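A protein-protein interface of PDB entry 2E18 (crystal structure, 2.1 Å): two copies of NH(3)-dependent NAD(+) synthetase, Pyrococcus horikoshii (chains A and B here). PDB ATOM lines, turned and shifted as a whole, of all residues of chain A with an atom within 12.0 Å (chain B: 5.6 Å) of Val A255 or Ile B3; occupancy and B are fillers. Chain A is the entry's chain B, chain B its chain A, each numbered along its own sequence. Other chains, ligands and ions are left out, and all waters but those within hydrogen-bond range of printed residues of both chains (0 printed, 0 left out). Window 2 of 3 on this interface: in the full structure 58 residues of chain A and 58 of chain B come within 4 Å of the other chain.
The backbone carbonyl oxygen (O) of Ile B3 lies within hydrogen-bond range of the backbone NH (N) of Val A255, 2.6 Å away.
The backbone carbonyl oxygen of Leu A253 sits at hydrogen-bond distance from the backbone NH of Asp B5.
Leu A253 touches Leu B4 (O to CA, 3.7 Å).
Ile A254 touches Arg B2 (CD1 to NH1, 3.8 Å).
O of Ile B3 touches CA of Ile A254, at 3.4 Å.
Leu B4 touches Ile A254 (CD2 to CG1, 3.4 Å).
Ser A249 touches none of the printed residues of chain B.
Of the printed residues of chain B, Leu A253 touches Leu B4 (3.7 Å) and Asp B5 (3.2 Å).
Printed residues of chain B within 4 Å of Ile A254: Arg B2 (3.8 Å), Ile B3 (3.4 Å) and Leu B4 (3.4 Å).
Of chain B, only Ile B3 (2.6 Å) comes within 4 Å of Val A255.
Arg B2 touches just one residue of chain A: Ile A254 (3.8 Å).
Of chain A, only Ile A254 (3.4 Å) and Val A255 (2.6 Å) come within 4 Å of Ile B3.
Asp B5 touches just one residue of chain A: Leu A253 (3.2 Å).
The nearest residue of chain B that does not touch Val A255 is Asp B5 (4.4 Å).
The nearest residue of chain A that does not touch Ile B3 is Leu A253 (4.1 Å).
Of the 8 printed residues of chain A, 3 touch a printed residue of chain B.
Hydrophobic or aromatic side chains of chain A within 4 Å of the printed part of chain B: Ile A254 and Val A255.
Among the printed residues, 6 pairs touch across the chains.
Among the printed residues, no Asp or Glu carboxylate lies within 4 Å of a Lys or Arg side-chain nitrogen of the other chain.
No position is printed for both chains.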
ATOM      1  N   SER A 249      22.961   4.606   0.067  1.00  0.00           N
ATOM      2  CA  SER A 249      22.626   5.648  -0.909  1.00  0.00           C
ATOM      3  C   SER A 249      21.526   6.553  -0.325  1.00  0.00           C
ATOM      4  O   SER A 249      20.794   6.129   0.565  1.00  0.00           O
ATOM      5  CB  SER A 249      22.148   4.987  -2.207  1.00  0.00           C
ATOM      6  OG  SER A 249      22.129   5.910  -3.279  1.00  0.00           O
ATOM      7  N   PHE A 250      21.396   7.784  -0.827  1.00  0.00           N
ATOM      8  CA  PHE A 250      20.398   8.717  -0.290  1.00  0.00           C
ATOM      9  C   PHE A 250      19.554   9.492  -1.314  1.00  0.00           C
ATOM     10  O   PHE A 250      19.021  10.559  -1.000  1.00  0.00           O
ATOM     11  CB  PHE A 250      21.098   9.726   0.626  1.00  0.00           C
ATOM     12  CG  PHE A 250      22.070   9.097   1.586  1.00  0.00           C
ATOM     13  CD1 PHE A 250      21.620   8.312   2.642  1.00  0.00           C
ATOM     14  CD2 PHE A 250      23.442   9.263   1.410  1.00  0.00           C
ATOM     15  CE1 PHE A 250      22.529   7.696   3.513  1.00  0.00           C
ATOM     16  CE2 PHE A 250      24.356   8.654   2.272  1.00  0.00           C
ATOM     17  CZ  PHE A 250      23.899   7.869   3.323  1.00  0.00           C
ATOM     18  N   GLU A 251      19.423   8.961  -2.526  1.00  0.00           N
ATOM     19  CA  GLU A 251      18.653   9.623  -3.579  1.00  0.00           C
ATOM     20  C   GLU A 251      17.221   9.998  -3.196  1.00  0.00           C
ATOM     21  O   GLU A 251      16.774  11.109  -3.474  1.00  0.00           O
ATOM     22  CB  GLU A 251      18.627   8.751  -4.836  1.00  0.00           C
ATOM     23  CG  GLU A 251      19.520   9.270  -5.950  1.00  0.00           C
ATOM     24  CD  GLU A 251      20.948   9.506  -5.489  1.00  0.00           C
ATOM     25  OE1 GLU A 251      21.618   8.523  -5.107  1.00  0.00           O
ATOM     26  OE2 GLU A 251      21.398  10.675  -5.505  1.00  0.00           O
ATOM     27  N   ASP A 252      16.510   9.076  -2.560  1.00  0.00           N
ATOM     28  CA  ASP A 252      15.129   9.328  -2.161  1.00  0.00           C
ATOM     29  C   ASP A 252      14.994  10.262  -0.963  1.00  0.00           C
ATOM     30  O   ASP A 252      13.893  10.703  -0.638  1.00  0.00           O
ATOM     31  CB  ASP A 252      14.428   8.007  -1.851  1.00  0.00           C
ATOM     32  CG  ASP A 252      15.138   7.214  -0.777  1.00  0.00           C
ATOM     33  OD1 ASP A 252      16.316   6.860  -0.989  1.00  0.00           O
ATOM     34  OD2 ASP A 252      14.520   6.950   0.276  1.00  0.00           O
ATOM     35  N   LEU A 253      16.107  10.572  -0.310  1.00  0.00           N
ATOM     36  CA  LEU A 253      16.065  11.446   0.854  1.00  0.00           C
ATOM     37  C   LEU A 253      16.495  12.867   0.523  1.00  0.00           C
ATOM     38  O   LEU A 253      16.522  13.739   1.391  1.00  0.00           O
ATOM     39  CB  LEU A 253      16.949  10.879   1.968  1.00  0.00           C
ATOM     40  CG  LEU A 253      16.560   9.497   2.498  1.00  0.00           C
ATOM     41  CD1 LEU A 253      17.535   9.077   3.582  1.00  0.00           C
ATOM     42  CD2 LEU A 253      15.141   9.537   3.051  1.00  0.00           C
ATOM     43  N   ILE A 254      16.825  13.096  -0.740  1.00  0.00           N
ATOM     44  CA  ILE A 254      17.243  14.415  -1.181  1.00  0.00           C
ATOM     45  C   ILE A 254      16.000  15.252  -1.442  1.00  0.00           C
ATOM     46  O   ILE A 254      15.179  14.910  -2.290  1.00  0.00           O
ATOM     47  CB  ILE A 254      18.072  14.334  -2.478  1.00  0.00           C
ATOM     48  CG1 ILE A 254      19.292  13.443  -2.254  1.00  0.00           C
ATOM     49  CG2 ILE A 254      18.508  15.735  -2.909  1.00  0.00           C
ATOM     50  CD1 ILE A 254      20.124  13.232  -3.496  1.00  0.00           C
ATOM     51  N   VAL A 255      15.863  16.343  -0.697  1.00  0.00           N
ATOM     52  CA  VAL A 255      14.722  17.233  -0.843  1.00  0.00           C
ATOM     53  C   VAL A 255      14.954  18.135  -2.049  1.00  0.00           C
ATOM     54  O   VAL A 255      15.732  19.089  -1.984  1.00  0.00           O
ATOM     55  CB  VAL A 255      14.536  18.108   0.414  1.00  0.00           C
ATOM     56  CG1 VAL A 255      13.315  18.995   0.254  1.00  0.00           C
ATOM     57  CG2 VAL A 255      14.401  17.224   1.646  1.00  0.00           C
ATOM     58  N   GLY A 256      14.286  17.814  -3.150  1.00  0.00           N
ATOM     59  CA  GLY A 256      14.425  18.596  -4.363  1.00  0.00           C
ATOM     60  C   GLY A 256      13.161  19.369  -4.679  1.00  0.00           C
ATOM     61  O   GLY A 256      12.269  19.434  -3.803  1.00  0.00           O
ATOM     62  N   MET B   1      23.316  24.057  -2.459  1.00  0.00           N
ATOM     63  CA  MET B   1      23.690  22.655  -2.469  1.00  0.00           C
ATOM     64  C   MET B   1      22.450  21.782  -2.337  1.00  0.00           C
ATOM     65  O   MET B   1      21.405  22.204  -1.860  1.00  0.00           O
ATOM     66  CB  MET B   1      24.633  22.412  -1.296  1.00  0.00           C
ATOM     67  CG  MET B   1      25.037  20.945  -1.182  1.00  0.00           C
ATOM     68  SD  MET B   1      26.078  20.422  -2.554  1.00  0.00           S
ATOM     69  CE  MET B   1      26.824  18.986  -1.765  1.00  0.00           C
ATOM     70  N   ARG B   2      22.568  20.541  -2.830  1.00  0.00           N
ATOM     71  CA  ARG B   2      21.452  19.633  -2.636  1.00  0.00           C
ATOM     72  C   ARG B   2      21.098  19.591  -1.154  1.00  0.00           C
ATOM     73  O   ARG B   2      21.942  19.737  -0.280  1.00  0.00           O
ATOM     74  CB  ARG B   2      21.878  18.247  -3.111  1.00  0.00           C
ATOM     75  CG  ARG B   2      22.754  17.528  -2.088  1.00  0.00           C
ATOM     76  CD  ARG B   2      23.001  16.065  -2.471  1.00  0.00           C
ATOM     77  NE  ARG B   2      23.813  15.395  -1.455  1.00  0.00           N
ATOM     78  CZ  ARG B   2      24.186  14.128  -1.710  1.00  0.00           C
ATOM     79  NH1 ARG B   2      23.825  13.545  -2.841  1.00  0.00           N
ATOM     80  NH2 ARG B   2      24.927  13.465  -0.817  1.00  0.00           N
ATOM     81  N   ILE B   3      19.791  19.447  -0.884  1.00  0.00           N
ATOM     82  CA  ILE B   3      19.360  19.382   0.506  1.00  0.00           C
ATOM     83  C   ILE B   3      18.925  17.969   0.889  1.00  0.00           C
ATOM     84  O   ILE B   3      18.095  17.350   0.236  1.00  0.00           O
ATOM     85  CB  ILE B   3      18.204  20.364   0.700  1.00  0.00           C
ATOM     86  CG1 ILE B   3      18.741  21.798   0.753  1.00  0.00           C
ATOM     87  CG2 ILE B   3      17.486  20.078   2.031  1.00  0.00           C
ATOM     88  CD1 ILE B   3      17.630  22.830   0.958  1.00  0.00           C
ATOM     89  N   LEU B   4      19.468  17.458   1.990  1.00  0.00           N
ATOM     90  CA  LEU B   4      19.112  16.134   2.481  1.00  0.00           C
ATOM     91  C   LEU B   4      18.266  16.251   3.733  1.00  0.00           C
ATOM     92  O   LEU B   4      18.308  17.264   4.430  1.00  0.00           O
ATOM     93  CB  LEU B   4      20.365  15.333   2.843  1.00  0.00           C
ATOM     94  CG  LEU B   4      21.444  15.031   1.807  1.00  0.00           C
ATOM     95  CD1 LEU B   4      22.559  14.232   2.484  1.00  0.00           C
ATOM     96  CD2 LEU B   4      20.853  14.251   0.652  1.00  0.00           C
ATOM     97  N   ASP B   5      17.499  15.203   4.008  1.00  0.00           N
ATOM     98  CA  ASP B   5      16.688  15.134   5.211  1.00  0.00           C
ATOM     99  C   ASP B   5      17.582  14.358   6.177  1.00  0.00           C
ATOM    100  O   ASP B   5      17.483  13.134   6.288  1.00  0.00           O
ATOM    101  CB  ASP B   5      15.395  14.362   4.954  1.00  0.00           C
ATOM    102  CG  ASP B   5      14.556  14.200   6.207  1.00  0.00           C
ATOM    103  OD1 ASP B   5      14.996  14.653   7.286  1.00  0.00           O
ATOM    104  OD2 ASP B   5      13.455  13.617   6.114  1.00  0.00           O
